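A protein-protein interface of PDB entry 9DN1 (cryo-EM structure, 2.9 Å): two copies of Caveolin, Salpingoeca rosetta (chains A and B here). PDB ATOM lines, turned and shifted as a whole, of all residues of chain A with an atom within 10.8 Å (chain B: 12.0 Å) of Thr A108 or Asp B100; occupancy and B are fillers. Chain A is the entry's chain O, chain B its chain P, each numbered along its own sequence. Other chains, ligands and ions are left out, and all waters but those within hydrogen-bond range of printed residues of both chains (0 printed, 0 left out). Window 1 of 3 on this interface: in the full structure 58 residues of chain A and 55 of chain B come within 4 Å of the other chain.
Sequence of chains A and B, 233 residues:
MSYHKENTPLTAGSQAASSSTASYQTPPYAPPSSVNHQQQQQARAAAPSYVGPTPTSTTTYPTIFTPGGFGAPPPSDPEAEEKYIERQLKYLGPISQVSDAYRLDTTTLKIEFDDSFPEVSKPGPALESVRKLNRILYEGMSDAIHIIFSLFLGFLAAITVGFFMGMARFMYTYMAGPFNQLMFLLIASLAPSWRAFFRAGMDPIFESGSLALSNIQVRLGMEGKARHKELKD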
ATOM      1  N   TYR A  84      17.598 -22.869 -28.068  1.00  0.00           N
ATOM      2  CA  TYR A  84      16.809 -21.651 -27.914  1.00  0.00           C
ATOM      3  C   TYR A  84      16.118 -21.277 -29.222  1.00  0.00           C
ATOM      4  O   TYR A  84      14.917 -20.976 -29.241  1.00  0.00           O
ATOM      5  CB  TYR A  84      17.708 -20.511 -27.435  1.00  0.00           C
ATOM      6  CG  TYR A  84      16.981 -19.206 -27.219  1.00  0.00           C
ATOM      7  CD1 TYR A  84      17.199 -18.123 -28.059  1.00  0.00           C
ATOM      8  CD2 TYR A  84      16.080 -19.055 -26.177  1.00  0.00           C
ATOM      9  CE1 TYR A  84      16.539 -16.929 -27.868  1.00  0.00           C
ATOM     10  CE2 TYR A  84      15.414 -17.863 -25.978  1.00  0.00           C
ATOM     11  CZ  TYR A  84      15.650 -16.804 -26.826  1.00  0.00           C
ATOM     12  OH  TYR A  84      14.989 -15.614 -26.632  1.00  0.00           O
ATOM     13  N   ILE A  95       1.805 -13.808 -26.931  1.00  0.00           N
ATOM     14  CA  ILE A  95       1.973 -14.642 -25.748  1.00  0.00           C
ATOM     15  C   ILE A  95       1.509 -13.974 -24.463  1.00  0.00           C
ATOM     16  O   ILE A  95       1.716 -14.531 -23.385  1.00  0.00           O
ATOM     17  CB  ILE A  95       3.441 -15.096 -25.604  1.00  0.00           C
ATOM     18  CG1 ILE A  95       4.362 -13.886 -25.435  1.00  0.00           C
ATOM     19  CG2 ILE A  95       3.861 -15.911 -26.811  1.00  0.00           C
ATOM     20  CD1 ILE A  95       5.783 -14.251 -25.082  1.00  0.00           C
ATOM     21  N   SER A  96       0.892 -12.796 -24.527  1.00  0.00           N
ATOM     22  CA  SER A  96       0.571 -12.070 -23.306  1.00  0.00           C
ATOM     23  C   SER A  96      -0.528 -12.783 -22.518  1.00  0.00           C
ATOM     24  O   SER A  96      -1.283 -13.604 -23.046  1.00  0.00           O
ATOM     25  CB  SER A  96       0.137 -10.641 -23.625  1.00  0.00           C
ATOM     26  OG  SER A  96      -1.051 -10.627 -24.396  1.00  0.00           O
ATOM     27  N   GLN A  97      -0.605 -12.452 -21.225  1.00  0.00           N
ATOM     28  CA  GLN A  97      -1.540 -13.080 -20.295  1.00  0.00           C
ATOM     29  C   GLN A  97      -2.436 -12.064 -19.596  1.00  0.00           C
ATOM     30  O   GLN A  97      -2.963 -12.349 -18.516  1.00  0.00           O
ATOM     31  CB  GLN A  97      -0.772 -13.899 -19.255  1.00  0.00           C
ATOM     32  CG  GLN A  97      -1.184 -15.355 -19.174  1.00  0.00           C
ATOM     33  CD  GLN A  97      -0.368 -16.128 -18.157  1.00  0.00           C
ATOM     34  OE1 GLN A  97       0.853 -15.992 -18.093  1.00  0.00           O
ATOM     35  NE2 GLN A  97      -1.042 -16.940 -17.352  1.00  0.00           N
ATOM     36  N   ARG A 103      -3.973 -14.488 -11.147  1.00  0.00           N
ATOM     37  CA  ARG A 103      -2.908 -15.462 -11.340  1.00  0.00           C
ATOM     38  C   ARG A 103      -1.763 -15.221 -10.364  1.00  0.00           C
ATOM     39  O   ARG A 103      -1.563 -14.103  -9.879  1.00  0.00           O
ATOM     40  CB  ARG A 103      -2.377 -15.405 -12.771  1.00  0.00           C
ATOM     41  CG  ARG A 103      -1.754 -14.073 -13.130  1.00  0.00           C
ATOM     42  CD  ARG A 103      -1.573 -13.940 -14.624  1.00  0.00           C
ATOM     43  NE  ARG A 103      -0.593 -12.915 -14.959  1.00  0.00           N
ATOM     44  CZ  ARG A 103      -0.886 -11.650 -15.232  1.00  0.00           C
ATOM     45  NH1 ARG A 103      -2.132 -11.207 -15.213  1.00  0.00           N
ATOM     46  NH2 ARG A 103       0.098 -10.807 -15.526  1.00  0.00           N
ATOM     47  N   LEU A 104      -1.012 -16.284 -10.085  1.00  0.00           N
ATOM     48  CA  LEU A 104       0.168 -16.219  -9.235  1.00  0.00           C
ATOM     49  C   LEU A 104       1.432 -16.081 -10.080  1.00  0.00           C
ATOM     50  O   LEU A 104       1.420 -16.265 -11.298  1.00  0.00           O
ATOM     51  CB  LEU A 104       0.276 -17.464  -8.352  1.00  0.00           C
ATOM     52  CG  LEU A 104      -0.870 -17.766  -7.385  1.00  0.00           C
ATOM     53  CD1 LEU A 104      -0.652 -19.115  -6.732  1.00  0.00           C
ATOM     54  CD2 LEU A 104      -0.988 -16.687  -6.327  1.00  0.00           C
ATOM     55  N   ASP A 105       2.537 -15.758  -9.406  1.00  0.00           N
ATOM     56  CA  ASP A 105       3.821 -15.518 -10.053  1.00  0.00           C
ATOM     57  C   ASP A 105       4.813 -16.658  -9.846  1.00  0.00           C
ATOM     58  O   ASP A 105       6.001 -16.489 -10.136  1.00  0.00           O
ATOM     59  CB  ASP A 105       4.429 -14.215  -9.530  1.00  0.00           C
ATOM     60  CG  ASP A 105       3.927 -12.992 -10.270  1.00  0.00           C
ATOM     61  OD1 ASP A 105       3.825 -11.922  -9.636  1.00  0.00           O
ATOM     62  OD2 ASP A 105       3.641 -13.094 -11.481  1.00  0.00           O
ATOM     63  N   THR A 106       4.356 -17.812  -9.360  1.00  0.00           N
ATOM     64  CA  THR A 106       5.288 -18.856  -8.944  1.00  0.00           C
ATOM     65  C   THR A 106       6.099 -19.407 -10.110  1.00  0.00           C
ATOM     66  O   THR A 106       7.215 -19.900  -9.907  1.00  0.00           O
ATOM     67  CB  THR A 106       4.528 -19.989  -8.252  1.00  0.00           C
ATOM     68  OG1 THR A 106       5.456 -20.972  -7.778  1.00  0.00           O
ATOM     69  CG2 THR A 106       3.538 -20.646  -9.209  1.00  0.00           C
ATOM     70  N   THR A 107       5.568 -19.340 -11.333  1.00  0.00           N
ATOM     71  CA  THR A 107       6.205 -20.030 -12.451  1.00  0.00           C
ATOM     72  C   THR A 107       7.545 -19.418 -12.845  1.00  0.00           C
ATOM     73  O   THR A 107       8.325 -20.073 -13.543  1.00  0.00           O
ATOM     74  CB  THR A 107       5.280 -20.047 -13.671  1.00  0.00           C
ATOM     75  OG1 THR A 107       5.957 -20.656 -14.777  1.00  0.00           O
ATOM     76  CG2 THR A 107       4.857 -18.635 -14.065  1.00  0.00           C
ATOM     77  N   THR A 108       7.833 -18.186 -12.419  1.00  0.00           N
ATOM     78  CA  THR A 108       9.063 -17.519 -12.835  1.00  0.00           C
ATOM     79  C   THR A 108      10.251 -17.839 -11.936  1.00  0.00           C
ATOM     80  O   THR A 108      11.394 -17.609 -12.342  1.00  0.00           O
ATOM     81  CB  THR A 108       8.854 -16.003 -12.865  1.00  0.00           C
ATOM     82  OG1 THR A 108       7.679 -15.692 -13.624  1.00  0.00           O
ATOM     83  CG2 THR A 108      10.052 -15.307 -13.491  1.00  0.00           C
ATOM     84  N   LEU A 109      10.015 -18.369 -10.742  1.00  0.00           N
ATOM     85  CA  LEU A 109      11.081 -18.538  -9.769  1.00  0.00           C
ATOM     86  C   LEU A 109      11.910 -19.780 -10.074  1.00  0.00           C
ATOM     87  O   LEU A 109      11.429 -20.745 -10.673  1.00  0.00           O
ATOM     88  CB  LEU A 109      10.500 -18.628  -8.360  1.00  0.00           C
ATOM     89  CG  LEU A 109       9.619 -17.440  -7.963  1.00  0.00           C
ATOM     90  CD1 LEU A 109       8.973 -17.678  -6.611  1.00  0.00           C
ATOM     91  CD2 LEU A 109      10.420 -16.150  -7.954  1.00  0.00           C
ATOM     92  N   LYS A 110      13.174 -19.743  -9.651  1.00  0.00           N
ATOM     93  CA  LYS A 110      14.118 -20.840  -9.875  1.00  0.00           C
ATOM     94  C   LYS A 110      15.021 -20.934  -8.650  1.00  0.00           C
ATOM     95  O   LYS A 110      15.895 -20.087  -8.450  1.00  0.00           O
ATOM     96  CB  LYS A 110      14.931 -20.623 -11.145  1.00  0.00           C
ATOM     97  CG  LYS A 110      14.185 -20.972 -12.422  1.00  0.00           C
ATOM     98  CD  LYS A 110      14.696 -20.176 -13.616  1.00  0.00           C
ATOM     99  CE  LYS A 110      13.567 -19.462 -14.344  1.00  0.00           C
ATOM    100  NZ  LYS A 110      14.071 -18.338 -15.182  1.00  0.00           N
ATOM    101  N   ILE A 111      14.813 -21.967  -7.841  1.00  0.00           N
ATOM    102  CA  ILE A 111      15.574 -22.186  -6.618  1.00  0.00           C
ATOM    103  C   ILE A 111      16.376 -23.465  -6.815  1.00  0.00           C
ATOM    104  O   ILE A 111      15.863 -24.573  -6.628  1.00  0.00           O
ATOM    105  CB  ILE A 111      14.666 -22.276  -5.387  1.00  0.00           C
ATOM    106  CG1 ILE A 111      13.896 -20.965  -5.194  1.00  0.00           C
ATOM    107  CG2 ILE A 111      15.480 -22.601  -4.147  1.00  0.00           C
ATOM    108  CD1 ILE A 111      14.777 -19.740  -5.020  1.00  0.00           C
ATOM    109  N   GLU A 112      17.641 -23.312  -7.195  1.00  0.00           N
ATOM    110  CA  GLU A 112      18.535 -24.444  -7.378  1.00  0.00           C
ATOM    111  C   GLU A 112      19.960 -23.923  -7.276  1.00  0.00           C
ATOM    112  O   GLU A 112      20.218 -22.737  -7.492  1.00  0.00           O
ATOM    113  CB  GLU A 112      18.283 -25.139  -8.721  1.00  0.00           C
ATOM    114  CG  GLU A 112      19.130 -26.375  -8.959  1.00  0.00           C
ATOM    115  CD  GLU A 112      18.550 -27.284 -10.028  1.00  0.00           C
ATOM    116  OE1 GLU A 112      17.354 -27.133 -10.358  1.00  0.00           O
ATOM    117  OE2 GLU A 112      19.287 -28.153 -10.536  1.00  0.00           O
ATOM    118  N   ASP A 115      21.487 -21.856  -9.897  1.00  0.00           N
ATOM    119  CA  ASP A 115      20.857 -20.550 -10.027  1.00  0.00           C
ATOM    120  C   ASP A 115      21.009 -19.688  -8.783  1.00  0.00           C
ATOM    121  O   ASP A 115      21.077 -18.461  -8.899  1.00  0.00           O
ATOM    122  CB  ASP A 115      19.368 -20.717 -10.343  1.00  0.00           C
ATOM    123  CG  ASP A 115      19.126 -21.573 -11.570  1.00  0.00           C
ATOM    124  OD1 ASP A 115      19.136 -21.027 -12.692  1.00  0.00           O
ATOM    125  OD2 ASP A 115      18.928 -22.796 -11.413  1.00  0.00           O
ATOM    126  N   ILE B  95      13.215 -10.621 -29.764  1.00  0.00           N
ATOM    127  CA  ILE B  95      14.128 -11.219 -28.799  1.00  0.00           C
ATOM    128  C   ILE B  95      13.986 -10.650 -27.395  1.00  0.00           C
ATOM    129  O   ILE B  95      14.786 -10.988 -26.523  1.00  0.00           O
ATOM    130  CB  ILE B  95      15.590 -11.084 -29.273  1.00  0.00           C
ATOM    131  CG1 ILE B  95      15.977  -9.609 -29.405  1.00  0.00           C
ATOM    132  CG2 ILE B  95      15.781 -11.797 -30.598  1.00  0.00           C
ATOM    133  CD1 ILE B  95      17.444  -9.388 -29.668  1.00  0.00           C
ATOM    134  N   SER B  96      13.001  -9.792 -27.137  1.00  0.00           N
ATOM    135  CA  SER B  96      12.930  -9.122 -25.845  1.00  0.00           C
ATOM    136  C   SER B  96      12.574 -10.108 -24.733  1.00  0.00           C
ATOM    137  O   SER B  96      12.034 -11.192 -24.970  1.00  0.00           O
ATOM    138  CB  SER B  96      11.908  -7.987 -25.882  1.00  0.00           C
ATOM    139  OG  SER B  96      10.604  -8.481 -26.127  1.00  0.00           O
ATOM    140  N   GLN B  97      12.891  -9.709 -23.497  1.00  0.00           N
ATOM    141  CA  GLN B  97      12.701 -10.545 -22.315  1.00  0.00           C
ATOM    142  C   GLN B  97      11.835  -9.869 -21.255  1.00  0.00           C
ATOM    143  O   GLN B  97      11.916 -10.224 -20.076  1.00  0.00           O
ATOM    144  CB  GLN B  97      14.059 -10.919 -21.717  1.00  0.00           C
ATOM    145  CG  GLN B  97      14.358 -12.405 -21.720  1.00  0.00           C
ATOM    146  CD  GLN B  97      15.639 -12.734 -20.982  1.00  0.00           C
ATOM    147  OE1 GLN B  97      16.686 -12.139 -21.238  1.00  0.00           O
ATOM    148  NE2 GLN B  97      15.563 -13.683 -20.055  1.00  0.00           N
ATOM    149  N   VAL B  98      10.996  -8.907 -21.649  1.00  0.00           N
ATOM    150  CA  VAL B  98      10.226  -8.135 -20.680  1.00  0.00           C
ATOM    151  C   VAL B  98       9.160  -8.952 -19.967  1.00  0.00           C
ATOM    152  O   VAL B  98       8.608  -8.484 -18.966  1.00  0.00           O
ATOM    153  CB  VAL B  98       9.554  -6.924 -21.356  1.00  0.00           C
ATOM    154  CG1 VAL B  98      10.603  -5.938 -21.838  1.00  0.00           C
ATOM    155  CG2 VAL B  98       8.668  -7.371 -22.508  1.00  0.00           C
ATOM    156  N   SER B  99       8.854 -10.157 -20.448  1.00  0.00           N
ATOM    157  CA  SER B  99       7.800 -10.956 -19.833  1.00  0.00           C
ATOM    158  C   SER B  99       8.238 -11.608 -18.527  1.00  0.00           C
ATOM    159  O   SER B  99       7.408 -12.247 -17.871  1.00  0.00           O
ATOM    160  CB  SER B  99       7.320 -12.029 -20.813  1.00  0.00           C
ATOM    161  OG  SER B  99       8.398 -12.820 -21.284  1.00  0.00           O
ATOM    162  N   ASP B 100       9.506 -11.474 -18.139  1.00  0.00           N
ATOM    163  CA  ASP B 100      10.029 -12.048 -16.904  1.00  0.00           C
ATOM    164  C   ASP B 100      10.576 -10.907 -16.057  1.00  0.00           C
ATOM    165  O   ASP B 100      11.432 -10.146 -16.517  1.00  0.00           O
ATOM    166  CB  ASP B 100      11.110 -13.093 -17.211  1.00  0.00           C
ATOM    167  CG  ASP B 100      11.949 -13.490 -15.991  1.00  0.00           C
ATOM    168  OD1 ASP B 100      12.550 -14.585 -16.047  1.00  0.00           O
ATOM    169  OD2 ASP B 100      12.023 -12.754 -14.986  1.00  0.00           O
ATOM    170  N   ALA B 101      10.084 -10.796 -14.824  1.00  0.00           N
ATOM    171  CA  ALA B 101      10.469  -9.717 -13.927  1.00  0.00           C
ATOM    172  C   ALA B 101      11.445 -10.147 -12.839  1.00  0.00           C
ATOM    173  O   ALA B 101      11.801  -9.319 -11.995  1.00  0.00           O
ATOM    174  CB  ALA B 101       9.222  -9.119 -13.267  1.00  0.00           C
ATOM    175  N   TYR B 102      11.888 -11.402 -12.836  1.00  0.00           N
ATOM    176  CA  TYR B 102      12.676 -11.972 -11.747  1.00  0.00           C
ATOM    177  C   TYR B 102      13.965 -12.604 -12.260  1.00  0.00           C
ATOM    178  O   TYR B 102      14.278 -13.754 -11.945  1.00  0.00           O
ATOM    179  CB  TYR B 102      11.858 -12.999 -10.969  1.00  0.00           C
ATOM    180  CG  TYR B 102      10.574 -12.459 -10.385  1.00  0.00           C
ATOM    181  CD1 TYR B 102      10.587 -11.662  -9.250  1.00  0.00           C
ATOM    182  CD2 TYR B 102       9.347 -12.751 -10.963  1.00  0.00           C
ATOM    183  CE1 TYR B 102       9.416 -11.168  -8.711  1.00  0.00           C
ATOM    184  CE2 TYR B 102       8.173 -12.262 -10.431  1.00  0.00           C
ATOM    185  CZ  TYR B 102       8.213 -11.471  -9.306  1.00  0.00           C
ATOM    186  OH  TYR B 102       7.045 -10.980  -8.773  1.00  0.00           O
ATOM    187  N   ARG B 103      14.733 -11.865 -13.057  1.00  0.00           N
ATOM    188  CA  ARG B 103      15.920 -12.392 -13.714  1.00  0.00           C
ATOM    189  C   ARG B 103      17.171 -11.652 -13.257  1.00  0.00           C
ATOM    190  O   ARG B 103      17.108 -10.499 -12.821  1.00  0.00           O
ATOM    191  CB  ARG B 103      15.791 -12.280 -15.232  1.00  0.00           C
ATOM    192  CG  ARG B 103      15.679 -10.854 -15.725  1.00  0.00           C
ATOM    193  CD  ARG B 103      15.203 -10.808 -17.158  1.00  0.00           C
ATOM    194  NE  ARG B 103      15.512  -9.530 -17.786  1.00  0.00           N
ATOM    195  CZ  ARG B 103      14.682  -8.496 -17.840  1.00  0.00           C
ATOM    196  NH1 ARG B 103      13.474  -8.547 -17.305  1.00  0.00           N
ATOM    197  NH2 ARG B 103      15.077  -7.381 -18.446  1.00  0.00           N
ATOM    198  N   LEU B 104      18.311 -12.333 -13.361  1.00  0.00           N
ATOM    199  CA  LEU B 104      19.609 -11.754 -13.045  1.00  0.00           C
ATOM    200  C   LEU B 104      20.293 -11.241 -14.310  1.00  0.00           C
ATOM    201  O   LEU B 104      19.879 -11.531 -15.434  1.00  0.00           O
ATOM    202  CB  LEU B 104      20.512 -12.778 -12.354  1.00  0.00           C
ATOM    203  CG  LEU B 104      20.035 -13.391 -11.036  1.00  0.00           C
ATOM    204  CD1 LEU B 104      20.983 -14.493 -10.607  1.00  0.00           C
ATOM    205  CD2 LEU B 104      19.932 -12.339  -9.951  1.00  0.00           C
ATOM    206  N   ASP B 105      21.362 -10.471 -14.106  1.00  0.00           N
ATOM    207  CA  ASP B 105      22.104  -9.834 -15.188  1.00  0.00           C
ATOM    208  C   ASP B 105      23.447 -10.502 -15.463  1.00  0.00           C
ATOM    209  O   ASP B 105      24.274  -9.933 -16.180  1.00  0.00           O
ATOM    210  CB  ASP B 105      22.331  -8.355 -14.861  1.00  0.00           C
ATOM    211  CG  ASP B 105      21.148  -7.483 -15.234  1.00  0.00           C
ATOM    212  OD1 ASP B 105      20.159  -8.013 -15.780  1.00  0.00           O
ATOM    213  OD2 ASP B 105      21.211  -6.263 -14.981  1.00  0.00           O
ATOM    214  N   THR B 106      23.682 -11.696 -14.917  1.00  0.00           N
ATOM    215  CA  THR B 106      25.020 -12.277 -14.967  1.00  0.00           C
ATOM    216  C   THR B 106      25.460 -12.600 -16.390  1.00  0.00           C
ATOM    217  O   THR B 106      26.662 -12.625 -16.672  1.00  0.00           O
ATOM    218  CB  THR B 106      25.076 -13.538 -14.104  1.00  0.00           C
ATOM    219  OG1 THR B 106      26.411 -14.059 -14.096  1.00  0.00           O
ATOM    220  CG2 THR B 106      24.119 -14.604 -14.630  1.00  0.00           C
ATOM    221  N   THR B 107      24.514 -12.849 -17.299  1.00  0.00           N
ATOM    222  CA  THR B 107      24.879 -13.360 -18.618  1.00  0.00           C
ATOM    223  C   THR B 107      25.623 -12.338 -19.468  1.00  0.00           C
ATOM    224  O   THR B 107      26.254 -12.721 -20.458  1.00  0.00           O
ATOM    225  CB  THR B 107      23.631 -13.834 -19.370  1.00  0.00           C
ATOM    226  OG1 THR B 107      24.012 -14.346 -20.653  1.00  0.00           O
ATOM    227  CG2 THR B 107      22.636 -12.695 -19.561  1.00  0.00           C
ATOM    228  N   TYR B 172       6.382 -19.842   1.709  1.00  0.00           N
ATOM    229  CA  TYR B 172       5.735 -19.603   0.425  1.00  0.00           C
ATOM    230  C   TYR B 172       4.611 -20.598   0.190  1.00  0.00           C
ATOM    231  O   TYR B 172       3.516 -20.218  -0.244  1.00  0.00           O
ATOM    232  CB  TYR B 172       6.747 -19.678  -0.717  1.00  0.00           C
ATOM    233  CG  TYR B 172       6.174 -19.214  -2.037  1.00  0.00           C
ATOM    234  CD1 TYR B 172       6.088 -17.864  -2.341  1.00  0.00           C
ATOM    235  CD2 TYR B 172       5.704 -20.125  -2.973  1.00  0.00           C
ATOM    236  CE1 TYR B 172       5.560 -17.436  -3.542  1.00  0.00           C
ATOM    237  CE2 TYR B 172       5.174 -19.704  -4.177  1.00  0.00           C
ATOM    238  CZ  TYR B 172       5.105 -18.359  -4.456  1.00  0.00           C
ATOM    239  OH  TYR B 172       4.577 -17.933  -5.652  1.00  0.00           O
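OH of Tyr B102 is in hydrogen-bond range of OD1 of Asp A105 (3.5 Å).
The side-chain carboxylate of Asp B100 lies within hydrogen-bond range of the backbone NH of Tyr B102. O of Asp B100 sits at hydrogen-bond distance from NH1 of Arg B103 (2.7 Å).
Among the printed residues, pairs that only touch across the chains: Thr A106 with Tyr B172 (3.3 Å), Thr A108 with Asp B100 (3.6 Å) and Thr A108 with Tyr B102 (3.7 Å).
Thr A108 touches just these residues of chain B: Asp B100 (3.6 Å) and Tyr B102 (3.7 Å). Asp B100 touches just one residue of chain A: Thr A108. Asp A105 touches just one residue of chain B: Tyr B102 (3.5 Å). Of chain B, only Tyr B172 (3.3 Å) comes within 4 Å of Thr A106. Lys A110 touches none of the printed residues of chain B. No residue of chain A comes within 4 Å of Val B98. No residue of chain A comes within 4 Å of Ser B99. No residue of chain A comes within 4 Å of Ala B101. Tyr B102 touches just these residues of chain A: Asp A105 (3.5 Å) and Thr A108 (3.7 Å). No residue of chain A comes within 4 Å of Arg B103. Printed residues of chain A within 4 Å of Tyr B172: Thr A106. The nearest residue of chain A that does not touch Asp B100 is Lys A110 (4.1 Å). The nearest printed residue of chain A that does not touch Tyr B172 is Asp A105 (4.4 Å).
Of the 15 printed residues of chain A, 3 touch a printed residue of chain B. Printed residues of chain A that touch a printed residue of chain B: Asp A105, Thr A106 and Thr A108. Hydrophobic or aromatic side chains of chain B that line the printed part of chain A: Tyr B102 and Tyr B172.
8 positions are printed for both chains.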
